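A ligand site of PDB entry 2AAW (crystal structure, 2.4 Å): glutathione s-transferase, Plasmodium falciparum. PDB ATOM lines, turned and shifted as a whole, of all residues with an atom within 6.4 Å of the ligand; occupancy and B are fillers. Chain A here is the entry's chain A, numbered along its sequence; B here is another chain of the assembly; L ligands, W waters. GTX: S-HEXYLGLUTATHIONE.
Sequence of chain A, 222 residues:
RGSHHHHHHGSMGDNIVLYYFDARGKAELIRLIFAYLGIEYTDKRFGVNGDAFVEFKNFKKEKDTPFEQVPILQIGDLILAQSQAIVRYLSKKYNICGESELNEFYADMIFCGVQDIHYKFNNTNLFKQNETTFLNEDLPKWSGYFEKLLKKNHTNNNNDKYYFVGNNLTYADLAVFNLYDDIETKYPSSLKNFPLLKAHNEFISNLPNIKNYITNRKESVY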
ATOM      1  N   TYR A  20     -24.306   6.575   2.935  1.00  0.00           N
ATOM      2  CA  TYR A  20     -24.986   7.502   3.817  1.00  0.00           C
ATOM      3  C   TYR A  20     -25.921   6.699   4.712  1.00  0.00           C
ATOM      4  O   TYR A  20     -25.986   5.475   4.622  1.00  0.00           O
ATOM      5  CB  TYR A  20     -25.809   8.509   3.017  1.00  0.00           C
ATOM      6  CG  TYR A  20     -26.258   9.697   3.834  1.00  0.00           C
ATOM      7  CD1 TYR A  20     -25.329  10.511   4.498  1.00  0.00           C
ATOM      8  CD2 TYR A  20     -27.609  10.038   3.937  1.00  0.00           C
ATOM      9  CE1 TYR A  20     -25.732  11.622   5.232  1.00  0.00           C
ATOM     10  CE2 TYR A  20     -28.033  11.161   4.667  1.00  0.00           C
ATOM     11  CZ  TYR A  20     -27.085  11.947   5.316  1.00  0.00           C
ATOM     12  OH  TYR A  20     -27.490  13.072   6.010  1.00  0.00           O
ATOM     13  N   PHE A  21     -26.625   7.397   5.591  1.00  0.00           N
ATOM     14  CA  PHE A  21     -27.577   6.744   6.475  1.00  0.00           C
ATOM     15  C   PHE A  21     -28.879   6.571   5.690  1.00  0.00           C
ATOM     16  O   PHE A  21     -29.022   7.114   4.604  1.00  0.00           O
ATOM     17  CB  PHE A  21     -27.819   7.573   7.734  1.00  0.00           C
ATOM     18  CG  PHE A  21     -26.637   7.593   8.665  1.00  0.00           C
ATOM     19  CD1 PHE A  21     -25.710   8.634   8.609  1.00  0.00           C
ATOM     20  CD2 PHE A  21     -26.427   6.551   9.554  1.00  0.00           C
ATOM     21  CE1 PHE A  21     -24.585   8.624   9.429  1.00  0.00           C
ATOM     22  CE2 PHE A  21     -25.298   6.531  10.376  1.00  0.00           C
ATOM     23  CZ  PHE A  21     -24.377   7.568  10.314  1.00  0.00           C
ATOM     24  N   GLY A  25     -31.630  13.531   3.912  1.00  0.00           N
ATOM     25  CA  GLY A  25     -30.614  14.433   4.415  1.00  0.00           C
ATOM     26  C   GLY A  25     -29.671  15.106   3.433  1.00  0.00           C
ATOM     27  O   GLY A  25     -30.092  15.756   2.477  1.00  0.00           O
ATOM     28  N   LYS A  26     -28.376  14.940   3.682  1.00  0.00           N
ATOM     29  CA  LYS A  26     -27.346  15.555   2.858  1.00  0.00           C
ATOM     30  C   LYS A  26     -26.935  14.769   1.623  1.00  0.00           C
ATOM     31  O   LYS A  26     -26.018  15.181   0.912  1.00  0.00           O
ATOM     32  CB  LYS A  26     -26.120  15.832   3.721  1.00  0.00           C
ATOM     33  CG  LYS A  26     -26.377  16.790   4.873  1.00  0.00           C
ATOM     34  CD  LYS A  26     -25.085  17.195   5.551  1.00  0.00           C
ATOM     35  CE  LYS A  26     -25.329  18.245   6.626  1.00  0.00           C
ATOM     36  NZ  LYS A  26     -26.058  19.428   6.094  1.00  0.00           N
ATOM     37  N   PHE A  56     -21.908   1.862  10.108  1.00  0.00           N
ATOM     38  CA  PHE A  56     -21.176   3.115  10.061  1.00  0.00           C
ATOM     39  C   PHE A  56     -19.780   2.930  10.664  1.00  0.00           C
ATOM     40  O   PHE A  56     -18.781   3.352  10.068  1.00  0.00           O
ATOM     41  CB  PHE A  56     -21.948   4.199  10.829  1.00  0.00           C
ATOM     42  CG  PHE A  56     -21.305   5.553  10.766  1.00  0.00           C
ATOM     43  CD1 PHE A  56     -20.952   6.121   9.555  1.00  0.00           C
ATOM     44  CD2 PHE A  56     -21.053   6.258  11.945  1.00  0.00           C
ATOM     45  CE1 PHE A  56     -20.365   7.381   9.504  1.00  0.00           C
ATOM     46  CE2 PHE A  56     -20.460   7.522  11.901  1.00  0.00           C
ATOM     47  CZ  PHE A  56     -20.119   8.081  10.677  1.00  0.00           C
ATOM     48  N   LYS A  60     -16.083   3.306   8.529  1.00  0.00           N
ATOM     49  CA  LYS A  60     -14.926   4.166   8.783  1.00  0.00           C
ATOM     50  C   LYS A  60     -13.608   3.411   8.941  1.00  0.00           C
ATOM     51  O   LYS A  60     -12.536   4.006   8.808  1.00  0.00           O
ATOM     52  CB  LYS A  60     -15.183   5.038  10.010  1.00  0.00           C
ATOM     53  CG  LYS A  60     -16.304   6.030   9.807  1.00  0.00           C
ATOM     54  CD  LYS A  60     -16.444   6.991  10.968  1.00  0.00           C
ATOM     55  CE  LYS A  60     -17.026   6.313  12.197  1.00  0.00           C
ATOM     56  NZ  LYS A  60     -17.122   7.249  13.350  1.00  0.00           N
ATOM     57  N   GLU A  68     -14.219  11.626   8.591  1.00  0.00           N
ATOM     58  CA  GLU A  68     -15.037  10.646   9.294  1.00  0.00           C
ATOM     59  C   GLU A  68     -16.533  10.989   9.270  1.00  0.00           C
ATOM     60  O   GLU A  68     -17.252  10.768  10.249  1.00  0.00           O
ATOM     61  CB  GLU A  68     -14.561  10.488  10.753  1.00  0.00           C
ATOM     62  CG  GLU A  68     -13.114  10.018  10.882  1.00  0.00           C
ATOM     63  CD  GLU A  68     -12.685   9.743  12.330  1.00  0.00           C
ATOM     64  OE1 GLU A  68     -12.724  10.672  13.167  1.00  0.00           O
ATOM     65  OE2 GLU A  68     -12.307   8.597  12.630  1.00  0.00           O
ATOM     66  N   GLN A  69     -16.982  11.542   8.147  1.00  0.00           N
ATOM     67  CA  GLN A  69     -18.386  11.899   7.977  1.00  0.00           C
ATOM     68  C   GLN A  69     -18.894  11.373   6.639  1.00  0.00           C
ATOM     69  O   GLN A  69     -18.119  11.048   5.741  1.00  0.00           O
ATOM     70  CB  GLN A  69     -18.584  13.421   7.941  1.00  0.00           C
ATOM     71  CG  GLN A  69     -18.050  14.238   9.096  1.00  0.00           C
ATOM     72  CD  GLN A  69     -18.113  15.746   8.798  1.00  0.00           C
ATOM     73  OE1 GLN A  69     -17.547  16.218   7.806  1.00  0.00           O
ATOM     74  NE2 GLN A  69     -18.826  16.488   9.639  1.00  0.00           N
ATOM     75  N   VAL A  70     -20.215  11.271   6.525  1.00  0.00           N
ATOM     76  CA  VAL A  70     -20.852  10.851   5.285  1.00  0.00           C
ATOM     77  C   VAL A  70     -21.789  12.015   4.984  1.00  0.00           C
ATOM     78  O   VAL A  70     -22.119  12.790   5.884  1.00  0.00           O
ATOM     79  CB  VAL A  70     -21.659   9.524   5.425  1.00  0.00           C
ATOM     80  CG1 VAL A  70     -20.708   8.334   5.371  1.00  0.00           C
ATOM     81  CG2 VAL A  70     -22.445   9.512   6.727  1.00  0.00           C
ATOM     82  N   PRO A  71     -22.270  12.138   3.741  1.00  0.00           N
ATOM     83  CA  PRO A  71     -22.020  11.289   2.581  1.00  0.00           C
ATOM     84  C   PRO A  71     -20.582  11.146   2.099  1.00  0.00           C
ATOM     85  O   PRO A  71     -19.719  11.969   2.384  1.00  0.00           O
ATOM     86  CB  PRO A  71     -22.921  11.889   1.504  1.00  0.00           C
ATOM     87  CG  PRO A  71     -22.971  13.336   1.877  1.00  0.00           C
ATOM     88  CD  PRO A  71     -23.137  13.277   3.375  1.00  0.00           C
ATOM     89  N   ALA A  81     -15.563  13.202  -0.364  1.00  0.00           N
ATOM     90  CA  ALA A  81     -16.298  13.624   0.833  1.00  0.00           C
ATOM     91  C   ALA A  81     -16.828  15.051   0.702  1.00  0.00           C
ATOM     92  O   ALA A  81     -16.433  15.798  -0.206  1.00  0.00           O
ATOM     93  CB  ALA A  81     -15.383  13.527   2.044  1.00  0.00           C
ATOM     94  N   GLN A  82     -17.737  15.427   1.616  1.00  0.00           N
ATOM     95  CA  GLN A  82     -18.374  16.745   1.650  1.00  0.00           C
ATOM     96  C   GLN A  82     -19.417  16.913   0.531  1.00  0.00           C
ATOM     97  O   GLN A  82     -19.097  17.216  -0.618  1.00  0.00           O
ATOM     98  CB  GLN A  82     -17.320  17.847   1.584  1.00  0.00           C
ATOM     99  CG  GLN A  82     -16.412  17.901   2.820  1.00  0.00           C
ATOM    100  CD  GLN A  82     -17.117  18.465   4.074  1.00  0.00           C
ATOM    101  OE1 GLN A  82     -18.228  18.999   3.997  1.00  0.00           O
ATOM    102  NE2 GLN A  82     -16.470  18.358   5.224  1.00  0.00           N
ATOM    103  N   SER A  83     -20.677  16.731   0.897  1.00  0.00           N
ATOM    104  CA  SER A  83     -21.807  16.785  -0.026  1.00  0.00           C
ATOM    105  C   SER A  83     -21.848  17.932  -1.028  1.00  0.00           C
ATOM    106  O   SER A  83     -22.232  17.735  -2.187  1.00  0.00           O
ATOM    107  CB  SER A  83     -23.121  16.736   0.752  1.00  0.00           C
ATOM    108  OG  SER A  83     -23.296  17.877   1.570  1.00  0.00           O
ATOM    109  N   GLN A  84     -21.467  19.127  -0.600  1.00  0.00           N
ATOM    110  CA  GLN A  84     -21.495  20.281  -1.495  1.00  0.00           C
ATOM    111  C   GLN A  84     -20.376  20.233  -2.531  1.00  0.00           C
ATOM    112  O   GLN A  84     -20.568  20.636  -3.675  1.00  0.00           O
ATOM    113  CB  GLN A  84     -21.389  21.570  -0.694  1.00  0.00           C
ATOM    114  CG  GLN A  84     -22.410  21.671   0.412  1.00  0.00           C
ATOM    115  CD  GLN A  84     -22.357  23.019   1.084  1.00  0.00           C
ATOM    116  OE1 GLN A  84     -22.931  24.002   0.590  1.00  0.00           O
ATOM    117  NE2 GLN A  84     -21.663  23.091   2.217  1.00  0.00           N
ATOM    118  N   ILE A  86     -19.080  17.497  -3.611  1.00  0.00           N
ATOM    119  CA  ILE A  86     -19.481  16.402  -4.466  1.00  0.00           C
ATOM    120  C   ILE A  86     -20.475  16.906  -5.511  1.00  0.00           C
ATOM    121  O   ILE A  86     -20.299  16.683  -6.710  1.00  0.00           O
ATOM    122  CB  ILE A  86     -20.115  15.257  -3.637  1.00  0.00           C
ATOM    123  CG1 ILE A  86     -19.089  14.712  -2.641  1.00  0.00           C
ATOM    124  CG2 ILE A  86     -20.587  14.135  -4.560  1.00  0.00           C
ATOM    125  CD1 ILE A  86     -19.617  13.640  -1.718  1.00  0.00           C
ATOM    126  N   LEU A 126     -35.296  18.684  12.804  1.00  0.00           N
ATOM    127  CA  LEU A 126     -34.543  17.640  13.495  1.00  0.00           C
ATOM    128  C   LEU A 126     -34.144  17.919  14.941  1.00  0.00           C
ATOM    129  O   LEU A 126     -34.378  17.098  15.825  1.00  0.00           O
ATOM    130  CB  LEU A 126     -33.284  17.288  12.678  1.00  0.00           C
ATOM    131  CG  LEU A 126     -33.480  16.847  11.227  1.00  0.00           C
ATOM    132  CD1 LEU A 126     -32.131  16.411  10.646  1.00  0.00           C
ATOM    133  CD2 LEU A 126     -34.480  15.705  11.144  1.00  0.00           C
ATOM    134  N   PHE A 127     -33.558  19.085  15.191  1.00  0.00           N
ATOM    135  CA  PHE A 127     -33.112  19.445  16.534  1.00  0.00           C
ATOM    136  C   PHE A 127     -34.171  20.251  17.260  1.00  0.00           C
ATOM    137  O   PHE A 127     -33.875  21.033  18.171  1.00  0.00           O
ATOM    138  CB  PHE A 127     -31.796  20.224  16.426  1.00  0.00           C
ATOM    139  CG  PHE A 127     -30.875  19.655  15.387  1.00  0.00           C
ATOM    140  CD1 PHE A 127     -30.455  18.334  15.472  1.00  0.00           C
ATOM    141  CD2 PHE A 127     -30.493  20.412  14.295  1.00  0.00           C
ATOM    142  CE1 PHE A 127     -29.682  17.768  14.465  1.00  0.00           C
ATOM    143  CE2 PHE A 127     -29.718  19.856  13.279  1.00  0.00           C
ATOM    144  CZ  PHE A 127     -29.311  18.529  13.365  1.00  0.00           C
ATOM    145  N   TYR A 222     -36.614  12.896   7.464  1.00  0.00           N
ATOM    146  CA  TYR A 222     -35.396  13.584   7.062  1.00  0.00           C
ATOM    147  C   TYR A 222     -34.629  12.777   6.012  1.00  0.00           C
ATOM    148  O   TYR A 222     -34.938  11.570   5.833  1.00  0.00           O
ATOM    149  CB  TYR A 222     -34.524  13.859   8.301  1.00  0.00           C
ATOM    150  CG  TYR A 222     -33.196  13.140   8.393  1.00  0.00           C
ATOM    151  CD1 TYR A 222     -32.077  13.572   7.675  1.00  0.00           C
ATOM    152  CD2 TYR A 222     -33.040  12.037   9.236  1.00  0.00           C
ATOM    153  CE1 TYR A 222     -30.838  12.926   7.786  1.00  0.00           C
ATOM    154  CE2 TYR A 222     -31.803  11.381   9.357  1.00  0.00           C
ATOM    155  CZ  TYR A 222     -30.710  11.833   8.633  1.00  0.00           C
ATOM    156  OH  TYR A 222     -29.508  11.186   8.766  1.00  0.00           O
ATOM    157  OXT TYR A 222     -33.729  13.366   5.364  1.00  0.00           O
ATOM    158  N   CYS B 112     -14.722  23.015   2.528  1.00  0.00           N
ATOM    159  CA  CYS B 112     -15.966  22.624   3.199  1.00  0.00           C
ATOM    160  C   CYS B 112     -15.648  22.115   4.607  1.00  0.00           C
ATOM    161  O   CYS B 112     -16.397  22.361   5.552  1.00  0.00           O
ATOM    162  CB  CYS B 112     -16.714  21.539   2.394  1.00  0.00           C
ATOM    163  SG  CYS B 112     -17.458  22.157   0.839  1.00  0.00           S
ATOM    164  N   GLY B 113     -14.538  21.398   4.738  1.00  0.00           N
ATOM    165  CA  GLY B 113     -14.137  20.896   6.045  1.00  0.00           C
ATOM    166  C   GLY B 113     -13.826  22.072   6.959  1.00  0.00           C
ATOM    167  O   GLY B 113     -14.205  22.073   8.122  1.00  0.00           O
ATOM    168  N   ASP B 116     -16.960  23.262   8.523  1.00  0.00           N
ATOM    169  CA  ASP B 116     -17.524  22.509   9.632  1.00  0.00           C
ATOM    170  C   ASP B 116     -16.868  22.893  10.974  1.00  0.00           C
ATOM    171  O   ASP B 116     -17.568  23.139  11.963  1.00  0.00           O
ATOM    172  CB  ASP B 116     -17.391  20.997   9.397  1.00  0.00           C
ATOM    173  CG  ASP B 116     -18.294  20.490   8.256  1.00  0.00           C
ATOM    174  OD1 ASP B 116     -19.391  21.039   8.060  1.00  0.00           O
ATOM    175  OD2 ASP B 116     -17.912  19.512   7.560  1.00  0.00           O
ATOM    176  N   LYS B 141      -9.498  16.955  17.228  1.00  0.00           N
ATOM    177  CA  LYS B 141      -9.909  16.030  16.186  1.00  0.00           C
ATOM    178  C   LYS B 141      -9.751  16.594  14.776  1.00  0.00           C
ATOM    179  O   LYS B 141      -9.074  15.993  13.934  1.00  0.00           O
ATOM    180  CB  LYS B 141     -11.361  15.588  16.423  1.00  0.00           C
ATOM    181  CG  LYS B 141     -11.803  14.473  15.514  1.00  0.00           C
ATOM    182  CD  LYS B 141     -13.136  13.882  15.943  1.00  0.00           C
ATOM    183  CE  LYS B 141     -14.231  14.917  15.934  1.00  0.00           C
ATOM    184  NZ  LYS B 141     -15.545  14.325  16.314  1.00  0.00           N
HETATM  185  N1  GTX L   1     -20.343  19.268   5.798  1.00  0.00           N
HETATM  186  CA1 GTX L   1     -20.513  17.789   5.723  1.00  0.00           C
HETATM  187  C1  GTX L   1     -21.269  17.438   4.393  1.00  0.00           C
HETATM  188  O11 GTX L   1     -22.120  18.260   4.000  1.00  0.00           O
HETATM  189  O12 GTX L   1     -20.992  16.383   3.790  1.00  0.00           O
HETATM  190  CB1 GTX L   1     -21.273  17.375   7.002  1.00  0.00           C
HETATM  191  CG1 GTX L   1     -21.494  15.827   7.041  1.00  0.00           C
HETATM  192  CD1 GTX L   1     -22.233  15.437   8.330  1.00  0.00           C
HETATM  193  OE1 GTX L   1     -22.606  16.196   9.203  1.00  0.00           O
HETATM  194  N2  GTX L   1     -22.424  14.055   8.379  1.00  0.00           N
HETATM  195  CA2 GTX L   1     -23.072  13.397   9.487  1.00  0.00           C
HETATM  196  C2  GTX L   1     -22.069  12.327   9.907  1.00  0.00           C
HETATM  197  O2  GTX L   1     -21.504  11.534   9.168  1.00  0.00           O
HETATM  198  CB2 GTX L   1     -24.362  12.697   9.016  1.00  0.00           C
HETATM  199  SG2 GTX L   1     -25.605  13.890   8.507  1.00  0.00           S
HETATM  200  C1S GTX L   1     -27.110  13.229   9.215  1.00  0.00           C
HETATM  201  C2S GTX L   1     -27.843  14.321  10.033  1.00  0.00           C
HETATM  202  C3S GTX L   1     -27.946  13.914  11.512  1.00  0.00           C
HETATM  203  C4S GTX L   1     -28.017  15.177  12.393  1.00  0.00           C
HETATM  204  C5S GTX L   1     -27.310  14.966  13.760  1.00  0.00           C
HETATM  205  C6S GTX L   1     -26.550  16.247  14.135  1.00  0.00           C
HETATM  206  N3  GTX L   1     -21.887  12.364  11.313  1.00  0.00           N
HETATM  207  CA3 GTX L   1     -20.964  11.420  11.972  1.00  0.00           C
HETATM  208  C3  GTX L   1     -20.354  12.075  13.198  1.00  0.00           C
HETATM  209  O31 GTX L   1     -19.554  11.356  13.865  1.00  0.00           O
HETATM  210  O32 GTX L   1     -20.587  13.244  13.554  1.00  0.00           O
HETATM  211  O   HOH W   1     -22.869  14.921  12.885  1.00  0.00           O
HETATM  212  O   HOH W   2     -20.496  20.166   2.222  1.00  0.00           O
HETATM  213  O   HOH W   3     -17.585   9.955  12.986  1.00  0.00           O
HETATM  214  O   HOH W   4     -23.508  16.662  14.731  1.00  0.00           O
HETATM  215  O   HOH W   5     -19.192  14.180   3.938  1.00  0.00           O
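OD2 of Asp 116 of chain B sits at hydrogen-bond distance from NE2 of Gln 82, 3.0 Å away. The chain-end carboxylate (OXT) of Tyr 222 sits at hydrogen-bond distance from the backbone NH (N) of Gly 25. The side-chain hydroxyl (OH) of Tyr 20 lies within hydrogen-bond range of the backbone NH (N) of Lys 26. The side-chain carboxylate of Asp 116 of chain B sits close to the side-chain amide oxygen of Gln 69 (3.3 Å).
CD of Lys 26 touches O11 of the ligand, at 3.5 Å. CZ of Phe 56 touches CA3 of the ligand, at 3.7 Å. CA of Gln 69 touches O2 of the ligand, at 3.4 Å. Pro 71 touches the ligand. Phe 127 touches the ligand (CE1 to C6S, 3.5 Å). Tyr 222 touches the ligand. Within 4 Å of the ligand: Tyr 20, Lys 26, Phe 56, Gln 69, Val 70, Pro 71, Gln 82, Ser 83, Phe 127, Tyr 222 and Asp 116 of chain B. The nearest printed residue that does not touch the ligand is Phe 21 (4.1 Å).
Water W3 lies within hydrogen-bond range of an oxygen (O31) of the ligand (2.6 Å), the side-chain amino group of Lys 60 (2.8 Å) and the backbone carbonyl oxygen of Glu 68 (2.9 Å). Water W5 lies within hydrogen-bond range of the backbone carbonyl oxygen of Pro 71 (2.8 Å), an oxygen (O12) of the ligand (2.8 Å) and the backbone NH of Gln 82 (3.0 Å). Water W2 lies within hydrogen-bond range of O11 of the ligand (3.1 Å), OE1 of Gln 82 (3.1 Å) and NE2 of Gln 84 (3.1 Å).
An oxygen (O2) of the ligand lies within hydrogen-bond range of the backbone NH (N) of Val 70 (3.0 Å). OG of Ser 83 sits at hydrogen-bond distance from O11 of the ligand. The side-chain carboxylate (OD2) of Asp 116 of chain B lies within salt-bridge range of a nitrogen (N1) of the ligand (3.0 Å). An oxygen (O12) of the ligand sits at hydrogen-bond distance from the backbone NH (N) of Ser 83. N1 of the ligand is in hydrogen-bond range of OE1 of Gln 82 (2.8 Å). O of Val 70 lies within hydrogen-bond range of N2 of the ligand (2.8 Å). A sulfur (SG2) of the ligand sits close to the side-chain hydroxyl (OH) of Tyr 20 (3.2 Å).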
